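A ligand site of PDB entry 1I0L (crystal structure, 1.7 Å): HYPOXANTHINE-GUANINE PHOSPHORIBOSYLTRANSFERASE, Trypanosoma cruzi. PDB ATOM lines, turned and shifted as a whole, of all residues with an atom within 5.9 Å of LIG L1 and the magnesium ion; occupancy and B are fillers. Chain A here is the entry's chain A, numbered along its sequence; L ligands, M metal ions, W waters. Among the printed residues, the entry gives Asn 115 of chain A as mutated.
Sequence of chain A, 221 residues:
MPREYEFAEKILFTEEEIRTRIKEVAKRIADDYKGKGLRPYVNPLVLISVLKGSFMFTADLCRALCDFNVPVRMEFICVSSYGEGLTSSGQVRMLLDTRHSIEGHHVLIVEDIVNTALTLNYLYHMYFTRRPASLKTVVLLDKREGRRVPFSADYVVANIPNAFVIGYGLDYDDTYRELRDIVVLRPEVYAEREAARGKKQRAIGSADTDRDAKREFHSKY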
ATOM      1  N   VAL A  50     -12.840 -13.131  -1.343  1.00  0.00           N
ATOM      2  CA  VAL A  50     -12.520 -14.236  -2.218  1.00  0.00           C
ATOM      3  C   VAL A  50     -11.847 -13.734  -3.506  1.00  0.00           C
ATOM      4  O   VAL A  50     -12.461 -13.046  -4.327  1.00  0.00           O
ATOM      5  CB  VAL A  50     -13.794 -15.062  -2.530  1.00  0.00           C
ATOM      6  CG1 VAL A  50     -13.422 -16.344  -3.299  1.00  0.00           C
ATOM      7  CG2 VAL A  50     -14.545 -15.393  -1.236  1.00  0.00           C
ATOM      8  N   LEU A  51     -10.566 -14.057  -3.654  1.00  0.00           N
ATOM      9  CA  LEU A  51      -9.832 -13.642  -4.841  1.00  0.00           C
ATOM     10  C   LEU A  51     -10.333 -14.416  -6.058  1.00  0.00           C
ATOM     11  O   LEU A  51     -10.877 -15.507  -5.891  1.00  0.00           O
ATOM     12  CB  LEU A  51      -8.338 -13.919  -4.643  1.00  0.00           C
ATOM     13  CG  LEU A  51      -7.669 -13.089  -3.562  1.00  0.00           C
ATOM     14  CD1 LEU A  51      -6.240 -13.591  -3.377  1.00  0.00           C
ATOM     15  CD2 LEU A  51      -7.730 -11.600  -3.939  1.00  0.00           C
ATOM     16  N   LYS A  52     -10.132 -13.886  -7.272  1.00  0.00           N
ATOM     17  CA  LYS A  52      -9.484 -12.586  -7.485  1.00  0.00           C
ATOM     18  C   LYS A  52     -10.533 -11.476  -7.684  1.00  0.00           C
ATOM     19  O   LYS A  52     -10.287 -10.327  -7.359  1.00  0.00           O
ATOM     20  CB  LYS A  52      -8.629 -12.617  -8.748  1.00  0.00           C
ATOM     21  CG  LYS A  52      -7.500 -13.619  -8.823  1.00  0.00           C
ATOM     22  CD  LYS A  52      -6.711 -13.244 -10.060  1.00  0.00           C
ATOM     23  CE  LYS A  52      -5.869 -14.359 -10.626  1.00  0.00           C
ATOM     24  NZ  LYS A  52      -5.199 -13.879 -11.883  1.00  0.00           N
ATOM     25  N   GLY A  53     -11.702 -11.860  -8.206  1.00  0.00           N
ATOM     26  CA  GLY A  53     -12.756 -10.914  -8.499  1.00  0.00           C
ATOM     27  C   GLY A  53     -13.190  -9.881  -7.483  1.00  0.00           C
ATOM     28  O   GLY A  53     -13.492  -8.741  -7.849  1.00  0.00           O
ATOM     29  N   SER A  54     -13.170 -10.213  -6.203  1.00  0.00           N
ATOM     30  CA  SER A  54     -13.622  -9.250  -5.211  1.00  0.00           C
ATOM     31  C   SER A  54     -12.581  -8.227  -4.761  1.00  0.00           C
ATOM     32  O   SER A  54     -12.869  -7.414  -3.883  1.00  0.00           O
ATOM     33  CB  SER A  54     -14.187 -10.002  -4.005  1.00  0.00           C
ATOM     34  OG  SER A  54     -13.135 -10.642  -3.320  1.00  0.00           O
ATOM     35  N   GLU A 111     -17.846 -11.384  -1.954  1.00  0.00           N
ATOM     36  CA  GLU A 111     -17.759 -11.984  -3.287  1.00  0.00           C
ATOM     37  C   GLU A 111     -18.270 -10.958  -4.274  1.00  0.00           C
ATOM     38  O   GLU A 111     -19.057 -10.096  -3.896  1.00  0.00           O
ATOM     39  CB  GLU A 111     -18.613 -13.249  -3.367  1.00  0.00           C
ATOM     40  CG  GLU A 111     -17.816 -14.541  -3.391  1.00  0.00           C
ATOM     41  CD  GLU A 111     -17.068 -14.768  -4.709  1.00  0.00           C
ATOM     42  OE1 GLU A 111     -17.067 -15.938  -5.160  1.00  0.00           O
ATOM     43  OE2 GLU A 111     -16.477 -13.821  -5.304  1.00  0.00           O
ATOM     44  N   ASP A 112     -17.838 -11.029  -5.523  1.00  0.00           N
ATOM     45  CA  ASP A 112     -18.353 -10.046  -6.449  1.00  0.00           C
ATOM     46  C   ASP A 112     -19.541 -10.496  -7.279  1.00  0.00           C
ATOM     47  O   ASP A 112     -20.364  -9.683  -7.693  1.00  0.00           O
ATOM     48  CB  ASP A 112     -17.254  -9.326  -7.272  1.00  0.00           C
ATOM     49  CG  ASP A 112     -16.510 -10.227  -8.197  1.00  0.00           C
ATOM     50  OD1 ASP A 112     -16.473 -11.456  -7.984  1.00  0.00           O
ATOM     51  OD2 ASP A 112     -15.914  -9.676  -9.157  1.00  0.00           O
ATOM     52  N   ILE A 113     -19.712 -11.805  -7.418  1.00  0.00           N
ATOM     53  CA  ILE A 113     -20.858 -12.271  -8.178  1.00  0.00           C
ATOM     54  C   ILE A 113     -21.313 -13.653  -7.695  1.00  0.00           C
ATOM     55  O   ILE A 113     -20.491 -14.469  -7.290  1.00  0.00           O
ATOM     56  CB  ILE A 113     -20.587 -12.277  -9.732  1.00  0.00           C
ATOM     57  CG1 ILE A 113     -21.911 -12.366 -10.517  1.00  0.00           C
ATOM     58  CG2 ILE A 113     -19.706 -13.439 -10.138  1.00  0.00           C
ATOM     59  CD1 ILE A 113     -21.768 -12.100 -12.032  1.00  0.00           C
ATOM     60  N   VAL A 114     -22.643 -13.828  -7.585  1.00  0.00           N
ATOM     61  CA  VAL A 114     -23.192 -15.136  -7.241  1.00  0.00           C
ATOM     62  C   VAL A 114     -24.231 -15.444  -8.307  1.00  0.00           C
ATOM     63  O   VAL A 114     -25.009 -14.587  -8.697  1.00  0.00           O
ATOM     64  CB  VAL A 114     -23.766 -15.178  -5.823  1.00  0.00           C
ATOM     65  CG1 VAL A 114     -24.857 -14.165  -5.665  1.00  0.00           C
ATOM     66  CG2 VAL A 114     -24.205 -16.614  -5.481  1.00  0.00           C
ATOM     67  N   ASN A 115     -24.084 -16.637  -8.881  1.00  0.00           N
ATOM     68  CA  ASN A 115     -24.925 -17.151  -9.951  1.00  0.00           C
ATOM     69  C   ASN A 115     -25.382 -18.568  -9.552  1.00  0.00           C
ATOM     70  O   ASN A 115     -26.406 -18.707  -8.855  1.00  0.00           O
ATOM     71  CB  ASN A 115     -24.131 -17.159 -11.255  1.00  0.00           C
ATOM     72  CG  ASN A 115     -24.936 -17.611 -12.439  1.00  0.00           C
ATOM     73  OD1 ASN A 115     -26.135 -17.383 -12.490  1.00  0.00           O
ATOM     74  ND2 ASN A 115     -24.294 -18.255 -13.405  1.00  0.00           N
ATOM     75  N   THR A 116     -24.606 -19.604  -9.911  1.00  0.00           N
ATOM     76  CA  THR A 116     -24.957 -21.002  -9.532  1.00  0.00           C
ATOM     77  C   THR A 116     -24.869 -21.200  -8.028  1.00  0.00           C
ATOM     78  O   THR A 116     -25.602 -22.028  -7.459  1.00  0.00           O
ATOM     79  CB  THR A 116     -24.033 -22.058 -10.168  1.00  0.00           C
ATOM     80  OG1 THR A 116     -22.697 -21.888  -9.678  1.00  0.00           O
ATOM     81  CG2 THR A 116     -24.059 -21.998 -11.668  1.00  0.00           C
ATOM     82  N   ALA A 117     -23.958 -20.446  -7.419  1.00  0.00           N
ATOM     83  CA  ALA A 117     -23.675 -20.441  -5.982  1.00  0.00           C
ATOM     84  C   ALA A 117     -23.035 -21.720  -5.444  1.00  0.00           C
ATOM     85  O   ALA A 117     -22.907 -21.869  -4.222  1.00  0.00           O
ATOM     86  CB  ALA A 117     -24.946 -20.102  -5.158  1.00  0.00           C
ATOM     87  N   LEU A 118     -22.581 -22.594  -6.332  1.00  0.00           N
ATOM     88  CA  LEU A 118     -21.986 -23.864  -5.906  1.00  0.00           C
ATOM     89  C   LEU A 118     -20.799 -23.717  -4.948  1.00  0.00           C
ATOM     90  O   LEU A 118     -20.853 -24.213  -3.826  1.00  0.00           O
ATOM     91  CB  LEU A 118     -21.611 -24.687  -7.129  1.00  0.00           C
ATOM     92  CG  LEU A 118     -22.810 -25.249  -7.900  1.00  0.00           C
ATOM     93  CD1 LEU A 118     -22.366 -25.829  -9.227  1.00  0.00           C
ATOM     94  CD2 LEU A 118     -23.501 -26.296  -7.023  1.00  0.00           C
ATOM     95  N   THR A 119     -19.786 -22.961  -5.361  1.00  0.00           N
ATOM     96  CA  THR A 119     -18.593 -22.762  -4.523  1.00  0.00           C
ATOM     97  C   THR A 119     -18.839 -21.845  -3.342  1.00  0.00           C
ATOM     98  O   THR A 119     -18.289 -22.025  -2.278  1.00  0.00           O
ATOM     99  CB  THR A 119     -17.416 -22.225  -5.379  1.00  0.00           C
ATOM    100  OG1 THR A 119     -17.758 -20.940  -5.904  1.00  0.00           O
ATOM    101  CG2 THR A 119     -17.156 -23.158  -6.553  1.00  0.00           C
ATOM    102  N   LYS A 143     -27.187 -12.985  -9.723  1.00  0.00           N
ATOM    103  CA  LYS A 143     -27.982 -13.495 -10.839  1.00  0.00           C
ATOM    104  C   LYS A 143     -28.932 -14.477 -10.125  1.00  0.00           C
ATOM    105  O   LYS A 143     -28.701 -15.692 -10.084  1.00  0.00           O
ATOM    106  CB  LYS A 143     -27.130 -14.224 -11.850  1.00  0.00           C
ATOM    107  CG  LYS A 143     -26.270 -13.323 -12.702  1.00  0.00           C
ATOM    108  CD  LYS A 143     -25.556 -14.118 -13.780  1.00  0.00           C
ATOM    109  CE  LYS A 143     -24.688 -13.210 -14.646  1.00  0.00           C
ATOM    110  NZ  LYS A 143     -23.854 -13.979 -15.607  1.00  0.00           N
ATOM    111  N   GLY A 169     -13.507  -5.771 -11.261  1.00  0.00           N
ATOM    112  CA  GLY A 169     -13.050  -7.025 -10.654  1.00  0.00           C
ATOM    113  C   GLY A 169     -13.456  -8.249 -11.455  1.00  0.00           C
ATOM    114  O   GLY A 169     -12.751  -9.259 -11.465  1.00  0.00           O
ATOM    115  N   LEU A 170     -14.543  -8.135 -12.199  1.00  0.00           N
ATOM    116  CA  LEU A 170     -15.048  -9.237 -12.995  1.00  0.00           C
ATOM    117  C   LEU A 170     -14.306  -9.338 -14.301  1.00  0.00           C
ATOM    118  O   LEU A 170     -14.169  -8.366 -15.028  1.00  0.00           O
ATOM    119  CB  LEU A 170     -16.545  -9.040 -13.278  1.00  0.00           C
ATOM    120  CG  LEU A 170     -17.398  -9.064 -12.014  1.00  0.00           C
ATOM    121  CD1 LEU A 170     -18.674  -8.294 -12.240  1.00  0.00           C
ATOM    122  CD2 LEU A 170     -17.688 -10.503 -11.641  1.00  0.00           C
ATOM    123  N   ASP A 171     -13.972 -10.568 -14.657  1.00  0.00           N
ATOM    124  CA  ASP A 171     -13.211 -10.809 -15.883  1.00  0.00           C
ATOM    125  C   ASP A 171     -13.793 -11.794 -16.857  1.00  0.00           C
ATOM    126  O   ASP A 171     -14.728 -12.551 -16.575  1.00  0.00           O
ATOM    127  CB  ASP A 171     -11.834 -11.397 -15.498  1.00  0.00           C
ATOM    128  CG  ASP A 171     -11.933 -12.847 -15.004  1.00  0.00           C
ATOM    129  OD1 ASP A 171     -12.649 -13.111 -14.000  1.00  0.00           O
ATOM    130  OD2 ASP A 171     -11.300 -13.733 -15.608  1.00  0.00           O
ATOM    131  N   TYR A 172     -13.210 -11.765 -18.041  1.00  0.00           N
ATOM    132  CA  TYR A 172     -13.491 -12.759 -19.017  1.00  0.00           C
ATOM    133  C   TYR A 172     -12.067 -13.152 -19.399  1.00  0.00           C
ATOM    134  O   TYR A 172     -11.307 -12.327 -19.913  1.00  0.00           O
ATOM    135  CB  TYR A 172     -14.203 -12.264 -20.265  1.00  0.00           C
ATOM    136  CG  TYR A 172     -14.226 -13.406 -21.249  1.00  0.00           C
ATOM    137  CD1 TYR A 172     -14.825 -14.620 -20.889  1.00  0.00           C
ATOM    138  CD2 TYR A 172     -13.445 -13.381 -22.414  1.00  0.00           C
ATOM    139  CE1 TYR A 172     -14.624 -15.762 -21.616  1.00  0.00           C
ATOM    140  CE2 TYR A 172     -13.241 -14.540 -23.155  1.00  0.00           C
ATOM    141  CZ  TYR A 172     -13.829 -15.725 -22.731  1.00  0.00           C
ATOM    142  OH  TYR A 172     -13.561 -16.926 -23.348  1.00  0.00           O
ATOM    143  N   ARG A 177     -10.832  -6.910 -15.758  1.00  0.00           N
ATOM    144  CA  ARG A 177     -11.081  -6.696 -14.335  1.00  0.00           C
ATOM    145  C   ARG A 177     -10.898  -5.226 -13.949  1.00  0.00           C
ATOM    146  O   ARG A 177     -11.562  -4.734 -13.015  1.00  0.00           O
ATOM    147  CB  ARG A 177     -10.116  -7.510 -13.478  1.00  0.00           C
ATOM    148  CG  ARG A 177     -10.054  -8.990 -13.724  1.00  0.00           C
ATOM    149  CD  ARG A 177      -9.418  -9.680 -12.522  1.00  0.00           C
ATOM    150  NE  ARG A 177      -9.227 -11.096 -12.775  1.00  0.00           N
ATOM    151  CZ  ARG A 177     -10.091 -12.053 -12.431  1.00  0.00           C
ATOM    152  NH1 ARG A 177     -11.236 -11.731 -11.808  1.00  0.00           N
ATOM    153  NH2 ARG A 177      -9.839 -13.317 -12.760  1.00  0.00           N
HETATM  154  C1  LIG L   1     -16.402 -16.732 -11.025  1.00  0.00           C
HETATM  155  C2  LIG L   1     -17.407 -15.873 -10.489  1.00  0.00           C
HETATM  156  C3  LIG L   1     -18.049 -16.776  -9.434  1.00  0.00           C
HETATM  157  C4  LIG L   1     -17.767 -18.182  -9.965  1.00  0.00           C
HETATM  158  C5  LIG L   1     -19.081 -18.841 -10.303  1.00  0.00           C
HETATM  159  O1  LIG L   1     -15.200 -16.807 -10.180  1.00  0.00           O
HETATM  160  O2  LIG L   1     -16.622 -14.760 -10.115  1.00  0.00           O
HETATM  161  O3  LIG L   1     -17.516 -16.498  -8.172  1.00  0.00           O
HETATM  162  O4  LIG L   1     -17.084 -17.908 -11.243  1.00  0.00           O
HETATM  163  O5  LIG L   1     -19.439 -18.948 -11.695  1.00  0.00           O
HETATM  164  P1  LIG L   1     -20.969 -19.466 -12.121  1.00  0.00           P
HETATM  165  O6  LIG L   1     -21.644 -19.514 -10.785  1.00  0.00           O
HETATM  166  O7  LIG L   1     -20.693 -20.738 -12.805  1.00  0.00           O
HETATM  167  O8  LIG L   1     -21.492 -18.472 -13.095  1.00  0.00           O
HETATM  168  P2  LIG L   1     -13.888 -17.071 -11.037  1.00  0.00           P
HETATM  169  O9  LIG L   1     -13.769 -18.498 -11.219  1.00  0.00           O
HETATM  170  O10 LIG L   1     -14.113 -16.411 -12.310  1.00  0.00           O
HETATM  171  O11 LIG L   1     -12.829 -16.481 -10.166  1.00  0.00           O
HETATM  172  P3  LIG L   1     -12.258 -15.089 -10.243  1.00  0.00           P
HETATM  173  O12 LIG L   1     -12.468 -14.535 -11.590  1.00  0.00           O
HETATM  174  O13 LIG L   1     -10.798 -15.138  -9.902  1.00  0.00           O
HETATM  175  O14 LIG L   1     -12.833 -14.228  -9.173  1.00  0.00           O
HETATM  176  C1  LG2 L   2     -19.105 -15.816 -13.228  1.00  0.00           C
HETATM  177  C2  LG2 L   2     -18.867 -14.604 -13.873  1.00  0.00           C
HETATM  178  N1  LG2 L   2     -17.695 -13.933 -13.950  1.00  0.00           N
HETATM  179  C3  LG2 L   2     -17.853 -12.762 -14.626  1.00  0.00           C
HETATM  180  N2  LG2 L   2     -19.045 -12.343 -15.160  1.00  0.00           N
HETATM  181  C4  LG2 L   2     -20.235 -13.039 -15.105  1.00  0.00           C
HETATM  182  O1  LG2 L   2     -21.212 -12.639 -15.689  1.00  0.00           O
HETATM  183  C5  LG2 L   2     -20.084 -14.217 -14.415  1.00  0.00           C
HETATM  184  N3  LG2 L   2     -21.011 -15.181 -14.100  1.00  0.00           N
HETATM  185  N4  LG2 L   2     -20.377 -16.074 -13.410  1.00  0.00           N
HETATM  186 MG    MG M   1     -13.546 -14.746 -13.174  1.00  0.00          MG
HETATM  187  O   HOH W   1     -15.107 -17.555  -6.762  1.00  0.00           O
HETATM  188  O   HOH W   2     -18.383 -21.107 -14.527  1.00  0.00           O
HETATM  189  O   HOH W   3     -16.296 -17.122 -14.813  1.00  0.00           O
HETATM  190  O   HOH W   4     -22.024 -18.557  -8.327  1.00  0.00           O
HETATM  191  O   HOH W   5      -9.523 -17.264  -8.671  1.00  0.00           O
HETATM  192  O   HOH W   6     -14.629 -15.138 -14.975  1.00  0.00           O
HETATM  193  O   HOH W   7     -12.024 -15.874 -13.856  1.00  0.00           O
HETATM  194  O   HOH W   8     -20.553 -23.110 -11.894  1.00  0.00           O
HETATM  195  O   HOH W   9     -14.178 -14.692  -6.912  1.00  0.00           O
HETATM  196  O   HOH W  10      -9.611 -16.564 -11.862  1.00  0.00           O
HETATM  197  O   HOH W  11     -19.771 -16.896  -5.998  1.00  0.00           O
HETATM  198  O   HOH W  12     -21.502 -18.215 -15.819  1.00  0.00           O
HETATM  199  O   HOH W  13     -15.126 -13.588 -12.678  1.00  0.00           O
HETATM  200  O   HOH W  14     -22.198 -21.600 -14.606  1.00  0.00           O
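Water W6 bridges the backbone carbonyl oxygen of Asp 171 (3.0 Å) and a nitrogen (N1) of LG2 L2 (3.5 Å). Water W8 bridges an oxygen (O7) of LIG L1 (2.5 Å) and the side-chain hydroxyl of Thr 116 (3.3 Å). Water W10 lies within hydrogen-bond range of O13 of LIG L1 (2.7 Å) and NH2 of Arg 177 (3.4 Å). Water W12 lies within hydrogen-bond range of an oxygen (O8) of LIG L1 and a nitrogen (N4) of LG2 L2. Water W1 bridges O3 of LIG L1 (3.0 Å) and OE1 of Glu 111 (3.0 Å). Water W11 lies within hydrogen-bond range of the backbone carbonyl oxygen (O) of Ile 113, the side-chain carboxylate (OE1) of Glu 111 and an oxygen (O3) of LIG L1.
The side-chain hydroxyl (OG1) of Thr 116 lies within hydrogen-bond range of an oxygen (O6) of LIG L1. The side-chain amino group of Lys 143 lies within hydrogen-bond range of an oxygen (O1) of LG2 L2, at 3.0 Å. N of Lys 52 sits at hydrogen-bond distance from O13 of LIG L1 (3.0 Å). O13 of LIG L1 lies within salt-bridge range of NH2 of Arg 177, at 3.5 Å. The side-chain carboxylate (OE1) of Glu 111 is in hydrogen-bond range of an oxygen (O3) of LIG L1 (3.1 Å). ND2 of Asn 115 sits at hydrogen-bond distance from O8 of LIG L1, 2.8 Å away. The backbone NH (N) of Thr 116 lies within hydrogen-bond range of an oxygen (O6) of LIG L1 (3.1 Å). The backbone NH of Gly 53 is in hydrogen-bond range of an oxygen (O14) of LIG L1.
Residues that only touch the magnesium ion: Arg 177 (3.99 Å). The nearest printed residue that does not touch the magnesium ion is Leu 170 (5.6 Å).
An oxygen (O8) of LIG L1 sits at hydrogen-bond distance from a nitrogen (N3) of LG2 L2.
Leu 51 touches LIG L1 (C to O13, 3.9 Å). OD1 of Asp 112 touches O2 of LIG L1 (3.9 Å). CG2 of Ile 113 touches O2 of LIG L1, 3.4 Å away. Hydrophobic or aromatic side chains that line LIG L1: Ile 113. Within 4 Å of LIG L1: Leu 51, Lys 52, Gly 53, Glu 111, Asp 112, Ile 113, Asn 115, Thr 116, Asp 171 and Arg 177.
The magnesium ion is bound by O12 of LIG L1 (1.9 Å), O10 of LIG L1 (2.0 Å), water W7 (2.0 Å), water W13 (2.0 Å), OD1 of Asp 171 (2.0 Å) and water W6 (2.1 Å). The magnesium ion has six donor atoms within binding distance.
OG1 of Thr 116 lies close to N of Leu 118 (3.4 Å). The backbone carbonyl oxygen of Arg 177 lies within hydrogen-bond range of the backbone NH of Gly 169, at 2.8 Å. The side-chain carboxylate of Asp 171 is in salt-bridge range of the guanidinium group of Arg 177, 3.2 Å away.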
